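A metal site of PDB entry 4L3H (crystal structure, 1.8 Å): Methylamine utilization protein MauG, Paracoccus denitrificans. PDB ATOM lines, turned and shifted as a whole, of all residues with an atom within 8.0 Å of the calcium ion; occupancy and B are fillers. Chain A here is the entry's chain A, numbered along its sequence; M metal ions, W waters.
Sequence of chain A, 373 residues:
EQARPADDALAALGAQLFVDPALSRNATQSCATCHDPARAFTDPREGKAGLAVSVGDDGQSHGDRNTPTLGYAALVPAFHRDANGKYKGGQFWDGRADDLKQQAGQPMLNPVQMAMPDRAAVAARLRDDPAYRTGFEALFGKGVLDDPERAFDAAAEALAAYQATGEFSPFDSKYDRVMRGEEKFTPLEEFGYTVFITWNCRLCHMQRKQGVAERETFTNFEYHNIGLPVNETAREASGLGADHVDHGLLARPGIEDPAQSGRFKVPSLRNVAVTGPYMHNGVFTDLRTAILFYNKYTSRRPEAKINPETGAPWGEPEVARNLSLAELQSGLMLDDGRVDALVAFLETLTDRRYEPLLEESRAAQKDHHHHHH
OG1 of Thr 275 is in hydrogen-bond range of O of Asn 271.
O of Asn 66 sits at hydrogen-bond distance from NE1 of Trp 93.
O of Leu 51 sits at hydrogen-bond distance from ND2 of Asn 66.
N of Asn 66 lies within hydrogen-bond range of O of His 280.
The side-chain hydroxyl (OG1) of Thr 275 lies within hydrogen-bond range of the backbone carbonyl oxygen (O) of Val 272 (3.3 Å).
The backbone carbonyl oxygen of Ala 52 sits close to the side-chain amide nitrogen of Asn 66 (3.2 Å).
The calcium ion is bound by the side-chain amide oxygen of Asn 66, the backbone carbonyl oxygen of Pro 277, the backbone carbonyl oxygen of Thr 275, water W2, water W3, water W4 and water W1.
Water W3 bridges O of Gly 276 and ND2 of Asn 66.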
ATOM      1  N   ARG A  39     -20.858   8.247  -6.859  1.00  0.00           N
ATOM      2  CA  ARG A  39     -21.199   7.009  -7.584  1.00  0.00           C
ATOM      3  C   ARG A  39     -22.692   6.886  -7.760  1.00  0.00           C
ATOM      4  O   ARG A  39     -23.274   5.858  -7.406  1.00  0.00           O
ATOM      5  CB  ARG A  39     -20.613   5.756  -6.911  1.00  0.00           C
ATOM      6  CG  ARG A  39     -20.509   4.580  -7.870  1.00  0.00           C
ATOM      7  CD  ARG A  39     -19.781   3.338  -7.334  1.00  0.00           C
ATOM      8  NE  ARG A  39     -20.280   2.142  -8.011  1.00  0.00           N
ATOM      9  CZ  ARG A  39     -19.538   1.224  -8.622  1.00  0.00           C
ATOM     10  NH1 ARG A  39     -18.202   1.299  -8.621  1.00  0.00           N
ATOM     11  NH2 ARG A  39     -20.140   0.196  -9.209  1.00  0.00           N
ATOM     12  N   THR A  42     -24.789   5.467  -5.015  1.00  0.00           N
ATOM     13  CA  THR A  42     -24.655   4.046  -4.670  1.00  0.00           C
ATOM     14  C   THR A  42     -23.359   3.871  -3.939  1.00  0.00           C
ATOM     15  O   THR A  42     -22.577   4.869  -3.832  1.00  0.00           O
ATOM     16  CB  THR A  42     -24.642   3.132  -5.908  1.00  0.00           C
ATOM     17  OG1 THR A  42     -23.517   3.423  -6.733  1.00  0.00           O
ATOM     18  CG2 THR A  42     -25.870   3.299  -6.708  1.00  0.00           C
ATOM     19  N   ASP A  43     -23.106   2.629  -3.491  1.00  0.00           N
ATOM     20  CA  ASP A  43     -22.046   2.363  -2.496  1.00  0.00           C
ATOM     21  C   ASP A  43     -20.766   1.849  -3.152  1.00  0.00           C
ATOM     22  O   ASP A  43     -20.719   0.725  -3.718  1.00  0.00           O
ATOM     23  CB  ASP A  43     -22.523   1.429  -1.384  1.00  0.00           C
ATOM     24  CG  ASP A  43     -21.562   1.346  -0.176  1.00  0.00           C
ATOM     25  OD1 ASP A  43     -20.449   1.989  -0.203  1.00  0.00           O
ATOM     26  OD2 ASP A  43     -21.941   0.622   0.802  1.00  0.00           O
ATOM     27  N   LEU A  51     -19.392  -5.647  -3.570  1.00  0.00           N
ATOM     28  CA  LEU A  51     -20.234  -4.462  -3.659  1.00  0.00           C
ATOM     29  C   LEU A  51     -21.708  -4.856  -3.735  1.00  0.00           C
ATOM     30  O   LEU A  51     -22.559  -3.987  -3.814  1.00  0.00           O
ATOM     31  CB  LEU A  51     -19.831  -3.645  -4.903  1.00  0.00           C
ATOM     32  CG  LEU A  51     -18.813  -2.503  -4.864  1.00  0.00           C
ATOM     33  CD1 LEU A  51     -17.953  -2.550  -3.625  1.00  0.00           C
ATOM     34  CD2 LEU A  51     -17.906  -2.553  -6.079  1.00  0.00           C
ATOM     35  N   ALA A  52     -22.003  -6.144  -3.688  1.00  0.00           N
ATOM     36  CA  ALA A  52     -23.357  -6.637  -3.822  1.00  0.00           C
ATOM     37  C   ALA A  52     -24.231  -6.067  -2.711  1.00  0.00           C
ATOM     38  O   ALA A  52     -25.375  -5.745  -2.925  1.00  0.00           O
ATOM     39  CB  ALA A  52     -23.406  -8.160  -3.832  1.00  0.00           C
ATOM     40  N   ARG A  65     -29.626  -6.842   0.267  1.00  0.00           N
ATOM     41  CA  ARG A  65     -29.901  -6.169  -1.020  1.00  0.00           C
ATOM     42  C   ARG A  65     -28.861  -5.124  -1.431  1.00  0.00           C
ATOM     43  O   ARG A  65     -28.178  -4.494  -0.594  1.00  0.00           O
ATOM     44  CB  ARG A  65     -31.301  -5.557  -0.976  1.00  0.00           C
ATOM     45  CG  ARG A  65     -32.390  -6.616  -0.815  1.00  0.00           C
ATOM     46  CD  ARG A  65     -33.738  -6.041  -1.036  1.00  0.00           C
ATOM     47  NE  ARG A  65     -34.824  -7.005  -0.768  1.00  0.00           N
ATOM     48  CZ  ARG A  65     -36.016  -6.664  -0.326  1.00  0.00           C
ATOM     49  NH1 ARG A  65     -36.292  -5.381  -0.126  1.00  0.00           N
ATOM     50  NH2 ARG A  65     -36.955  -7.582  -0.126  1.00  0.00           N
ATOM     51  N   ASN A  66     -28.735  -4.935  -2.737  1.00  0.00           N
ATOM     52  CA  ASN A  66     -27.792  -4.024  -3.372  1.00  0.00           C
ATOM     53  C   ASN A  66     -28.345  -2.644  -3.114  1.00  0.00           C
ATOM     54  O   ASN A  66     -29.561  -2.420  -3.166  1.00  0.00           O
ATOM     55  CB  ASN A  66     -27.728  -4.265  -4.879  1.00  0.00           C
ATOM     56  CG  ASN A  66     -26.751  -3.348  -5.590  1.00  0.00           C
ATOM     57  OD1 ASN A  66     -27.107  -2.632  -6.583  1.00  0.00           O
ATOM     58  ND2 ASN A  66     -25.519  -3.353  -5.111  1.00  0.00           N
ATOM     59  N   THR A  67     -27.443  -1.727  -2.773  1.00  0.00           N
ATOM     60  CA  THR A  67     -27.861  -0.375  -2.499  1.00  0.00           C
ATOM     61  C   THR A  67     -28.219   0.308  -3.803  1.00  0.00           C
ATOM     62  O   THR A  67     -27.344   0.464  -4.670  1.00  0.00           O
ATOM     63  CB  THR A  67     -26.723   0.395  -1.762  1.00  0.00           C
ATOM     64  OG1 THR A  67     -26.619  -0.089  -0.425  1.00  0.00           O
ATOM     65  CG2 THR A  67     -27.081   1.868  -1.712  1.00  0.00           C
ATOM     66  N   PRO A  68     -29.487   0.730  -3.970  1.00  0.00           N
ATOM     67  CA  PRO A  68     -29.855   1.372  -5.227  1.00  0.00           C
ATOM     68  C   PRO A  68     -29.512   2.874  -5.347  1.00  0.00           C
ATOM     69  O   PRO A  68     -29.350   3.596  -4.346  1.00  0.00           O
ATOM     70  CB  PRO A  68     -31.378   1.113  -5.278  1.00  0.00           C
ATOM     71  CG  PRO A  68     -31.730   1.306  -3.843  1.00  0.00           C
ATOM     72  CD  PRO A  68     -30.637   0.691  -3.052  1.00  0.00           C
ATOM     73  N   THR A  69     -29.423   3.361  -6.581  1.00  0.00           N
ATOM     74  CA  THR A  69     -29.316   4.796  -6.821  1.00  0.00           C
ATOM     75  C   THR A  69     -30.554   5.509  -6.267  1.00  0.00           C
ATOM     76  O   THR A  69     -31.707   4.975  -6.307  1.00  0.00           O
ATOM     77  CB  THR A  69     -29.183   5.111  -8.320  1.00  0.00           C
ATOM     78  OG1 THR A  69     -28.965   6.480  -8.505  1.00  0.00           O
ATOM     79  CG2 THR A  69     -30.518   4.731  -9.064  1.00  0.00           C
ATOM     80  N   TRP A  93     -36.548  -2.027  -3.105  1.00  0.00           N
ATOM     81  CA  TRP A  93     -36.716  -3.030  -4.133  1.00  0.00           C
ATOM     82  C   TRP A  93     -38.052  -3.813  -4.036  1.00  0.00           C
ATOM     83  O   TRP A  93     -38.491  -4.389  -5.028  1.00  0.00           O
ATOM     84  CB  TRP A  93     -35.587  -4.003  -4.105  1.00  0.00           C
ATOM     85  CG  TRP A  93     -34.272  -3.509  -4.555  1.00  0.00           C
ATOM     86  CD1 TRP A  93     -33.265  -3.100  -3.760  1.00  0.00           C
ATOM     87  CD2 TRP A  93     -33.801  -3.466  -5.867  1.00  0.00           C
ATOM     88  NE1 TRP A  93     -32.201  -2.802  -4.474  1.00  0.00           N
ATOM     89  CE2 TRP A  93     -32.463  -3.029  -5.792  1.00  0.00           C
ATOM     90  CE3 TRP A  93     -34.333  -3.815  -7.103  1.00  0.00           C
ATOM     91  CZ2 TRP A  93     -31.668  -2.859  -6.917  1.00  0.00           C
ATOM     92  CZ3 TRP A  93     -33.530  -3.639  -8.238  1.00  0.00           C
ATOM     93  CH2 TRP A  93     -32.203  -3.163  -8.132  1.00  0.00           C
ATOM     94  N   ASN A 271     -28.549   5.848 -15.254  1.00  0.00           N
ATOM     95  CA  ASN A 271     -27.326   5.601 -14.528  1.00  0.00           C
ATOM     96  C   ASN A 271     -26.949   4.120 -14.332  1.00  0.00           C
ATOM     97  O   ASN A 271     -26.040   3.789 -13.592  1.00  0.00           O
ATOM     98  CB  ASN A 271     -27.302   6.357 -13.203  1.00  0.00           C
ATOM     99  CG  ASN A 271     -27.186   7.856 -13.402  1.00  0.00           C
ATOM    100  OD1 ASN A 271     -26.406   8.307 -14.251  1.00  0.00           O
ATOM    101  ND2 ASN A 271     -27.927   8.661 -12.585  1.00  0.00           N
ATOM    102  N   VAL A 272     -27.644   3.219 -15.015  1.00  0.00           N
ATOM    103  CA  VAL A 272     -27.412   1.813 -14.781  1.00  0.00           C
ATOM    104  C   VAL A 272     -25.964   1.426 -15.052  1.00  0.00           C
ATOM    105  O   VAL A 272     -25.367   0.583 -14.358  1.00  0.00           O
ATOM    106  CB  VAL A 272     -28.404   0.917 -15.553  1.00  0.00           C
ATOM    107  CG1 VAL A 272     -28.213   1.024 -17.071  1.00  0.00           C
ATOM    108  CG2 VAL A 272     -28.282  -0.499 -15.063  1.00  0.00           C
ATOM    109  N   VAL A 274     -23.328   2.874 -14.274  1.00  0.00           N
ATOM    110  CA  VAL A 274     -22.315   3.211 -13.255  1.00  0.00           C
ATOM    111  C   VAL A 274     -22.749   2.727 -11.871  1.00  0.00           C
ATOM    112  O   VAL A 274     -22.080   3.008 -10.894  1.00  0.00           O
ATOM    113  CB  VAL A 274     -21.978   4.722 -13.271  1.00  0.00           C
ATOM    114  CG1 VAL A 274     -21.633   5.174 -14.689  1.00  0.00           C
ATOM    115  CG2 VAL A 274     -23.109   5.586 -12.751  1.00  0.00           C
ATOM    116  N   THR A 275     -23.850   1.959 -11.805  1.00  0.00           N
ATOM    117  CA  THR A 275     -24.360   1.498 -10.502  1.00  0.00           C
ATOM    118  C   THR A 275     -24.288  -0.004 -10.253  1.00  0.00           C
ATOM    119  O   THR A 275     -25.005  -0.557  -9.439  1.00  0.00           O
ATOM    120  CB  THR A 275     -25.763   1.989 -10.305  1.00  0.00           C
ATOM    121  OG1 THR A 275     -26.589   1.481 -11.371  1.00  0.00           O
ATOM    122  CG2 THR A 275     -25.733   3.494 -10.327  1.00  0.00           C
ATOM    123  N   GLY A 276     -23.421  -0.683 -10.953  1.00  0.00           N
ATOM    124  CA  GLY A 276     -23.196  -2.131 -10.688  1.00  0.00           C
ATOM    125  C   GLY A 276     -22.779  -2.319  -9.246  1.00  0.00           C
ATOM    126  O   GLY A 276     -22.322  -1.382  -8.564  1.00  0.00           O
ATOM    127  N   PRO A 277     -22.883  -3.535  -8.759  1.00  0.00           N
ATOM    128  CA  PRO A 277     -23.421  -4.700  -9.362  1.00  0.00           C
ATOM    129  C   PRO A 277     -24.971  -4.564  -9.492  1.00  0.00           C
ATOM    130  O   PRO A 277     -25.562  -3.558  -9.086  1.00  0.00           O
ATOM    131  CB  PRO A 277     -23.010  -5.811  -8.401  1.00  0.00           C
ATOM    132  CG  PRO A 277     -22.837  -5.160  -7.118  1.00  0.00           C
ATOM    133  CD  PRO A 277     -22.383  -3.793  -7.397  1.00  0.00           C
ATOM    134  N   TYR A 278     -25.596  -5.558 -10.098  1.00  0.00           N
ATOM    135  CA  TYR A 278     -26.939  -5.385 -10.608  1.00  0.00           C
ATOM    136  C   TYR A 278     -27.933  -6.329  -9.970  1.00  0.00           C
ATOM    137  O   TYR A 278     -27.576  -7.316  -9.315  1.00  0.00           O
ATOM    138  CB  TYR A 278     -26.934  -5.484 -12.140  1.00  0.00           C
ATOM    139  CG  TYR A 278     -26.084  -4.415 -12.761  1.00  0.00           C
ATOM    140  CD1 TYR A 278     -26.551  -3.108 -12.847  1.00  0.00           C
ATOM    141  CD2 TYR A 278     -24.763  -4.667 -13.158  1.00  0.00           C
ATOM    142  CE1 TYR A 278     -25.756  -2.113 -13.357  1.00  0.00           C
ATOM    143  CE2 TYR A 278     -23.970  -3.664 -13.675  1.00  0.00           C
ATOM    144  CZ  TYR A 278     -24.484  -2.406 -13.792  1.00  0.00           C
ATOM    145  OH  TYR A 278     -23.717  -1.427 -14.330  1.00  0.00           O
ATOM    146  N   MET A 279     -29.213  -5.962 -10.136  1.00  0.00           N
ATOM    147  CA  MET A 279     -30.332  -6.662  -9.547  1.00  0.00           C
ATOM    148  C   MET A 279     -30.388  -6.387  -8.064  1.00  0.00           C
ATOM    149  O   MET A 279     -29.466  -5.818  -7.436  1.00  0.00           O
ATOM    150  CB  MET A 279     -30.275  -8.161  -9.855  1.00  0.00           C
ATOM    151  CG  MET A 279     -30.188  -8.436 -11.344  1.00  0.00           C
ATOM    152  SD  MET A 279     -31.549  -7.736 -12.275  1.00  0.00           S
ATOM    153  CE  MET A 279     -31.034  -7.953 -13.982  1.00  0.00           C
ATOM    154  N   HIS A 280     -31.477  -6.833  -7.483  1.00  0.00           N
ATOM    155  CA  HIS A 280     -31.826  -6.490  -6.138  1.00  0.00           C
ATOM    156  C   HIS A 280     -30.774  -7.015  -5.160  1.00  0.00           C
ATOM    157  O   HIS A 280     -30.692  -6.549  -4.038  1.00  0.00           O
ATOM    158  CB  HIS A 280     -33.234  -7.015  -5.781  1.00  0.00           C
ATOM    159  CG  HIS A 280     -33.304  -8.518  -5.749  1.00  0.00           C
ATOM    160  ND1 HIS A 280     -33.853  -9.252  -6.760  1.00  0.00           N
ATOM    161  CD2 HIS A 280     -32.898  -9.397  -4.813  1.00  0.00           C
ATOM    162  CE1 HIS A 280     -33.779 -10.537  -6.464  1.00  0.00           C
ATOM    163  NE2 HIS A 280     -33.177 -10.659  -5.289  1.00  0.00           N
ATOM    164  N   ASN A 281     -30.008  -8.015  -5.579  1.00  0.00           N
ATOM    165  CA  ASN A 281     -29.043  -8.682  -4.698  1.00  0.00           C
ATOM    166  C   ASN A 281     -27.631  -8.513  -5.171  1.00  0.00           C
ATOM    167  O   ASN A 281     -26.716  -9.159  -4.637  1.00  0.00           O
ATOM    168  CB  ASN A 281     -29.393 -10.160  -4.504  1.00  0.00           C
ATOM    169  CG  ASN A 281     -29.449 -10.937  -5.817  1.00  0.00           C
ATOM    170  OD1 ASN A 281     -29.185 -10.413  -6.878  1.00  0.00           O
ATOM    171  ND2 ASN A 281     -29.898 -12.171  -5.739  1.00  0.00           N
ATOM    172  N   GLY A 282     -27.434  -7.663  -6.168  1.00  0.00           N
ATOM    173  CA  GLY A 282     -26.093  -7.371  -6.686  1.00  0.00           C
ATOM    174  C   GLY A 282     -25.401  -8.604  -7.231  1.00  0.00           C
ATOM    175  O   GLY A 282     -24.164  -8.653  -7.290  1.00  0.00           O
ATOM    176  N   VAL A 283     -26.190  -9.590  -7.657  1.00  0.00           N
ATOM    177  CA  VAL A 283     -25.640 -10.891  -8.038  1.00  0.00           C
ATOM    178  C   VAL A 283     -24.791 -10.799  -9.278  1.00  0.00           C
ATOM    179  O   VAL A 283     -23.876 -11.590  -9.443  1.00  0.00           O
ATOM    180  CB  VAL A 283     -26.755 -11.949  -8.283  1.00  0.00           C
ATOM    181  CG1 VAL A 283     -27.690 -11.516  -9.405  1.00  0.00           C
ATOM    182  CG2 VAL A 283     -26.170 -13.308  -8.630  1.00  0.00           C
ATOM    183  N   PHE A 284     -25.082  -9.879 -10.175  1.00  0.00           N
ATOM    184  CA  PHE A 284     -24.236  -9.713 -11.361  1.00  0.00           C
ATOM    185  C   PHE A 284     -23.401  -8.458 -11.234  1.00  0.00           C
ATOM    186  O   PHE A 284     -23.961  -7.388 -10.990  1.00  0.00           O
ATOM    187  CB  PHE A 284     -25.042  -9.620 -12.650  1.00  0.00           C
ATOM    188  CG  PHE A 284     -26.113 -10.658 -12.758  1.00  0.00           C
ATOM    189  CD1 PHE A 284     -25.801 -12.002 -12.577  1.00  0.00           C
ATOM    190  CD2 PHE A 284     -27.398 -10.306 -13.078  1.00  0.00           C
ATOM    191  CE1 PHE A 284     -26.761 -12.984 -12.689  1.00  0.00           C
ATOM    192  CE2 PHE A 284     -28.380 -11.290 -13.189  1.00  0.00           C
ATOM    193  CZ  PHE A 284     -28.059 -12.630 -12.988  1.00  0.00           C
ATOM    194  N   THR A 285     -22.099  -8.588 -11.459  1.00  0.00           N
ATOM    195  CA  THR A 285     -21.195  -7.451 -11.372  1.00  0.00           C
ATOM    196  C   THR A 285     -21.249  -6.629 -12.641  1.00  0.00           C
ATOM    197  O   THR A 285     -21.168  -5.402 -12.562  1.00  0.00           O
ATOM    198  CB  THR A 285     -19.727  -7.828 -11.132  1.00  0.00           C
ATOM    199  OG1 THR A 285     -19.181  -8.357 -12.346  1.00  0.00           O
ATOM    200  CG2 THR A 285     -19.576  -8.815  -9.965  1.00  0.00           C
HETATM  201 CA    CA M   1     -26.627  -1.743  -8.263  1.00  0.00          CA
HETATM  202  O   HOH W   1     -27.681  -0.861 -10.316  1.00  0.00           O
HETATM  203  O   HOH W   2     -27.326   0.405  -7.486  1.00  0.00           O
HETATM  204  O   HOH W   3     -24.696  -1.187  -6.952  1.00  0.00           O
HETATM  205  O   HOH W   4     -28.724  -2.995  -8.486  1.00  0.00           O
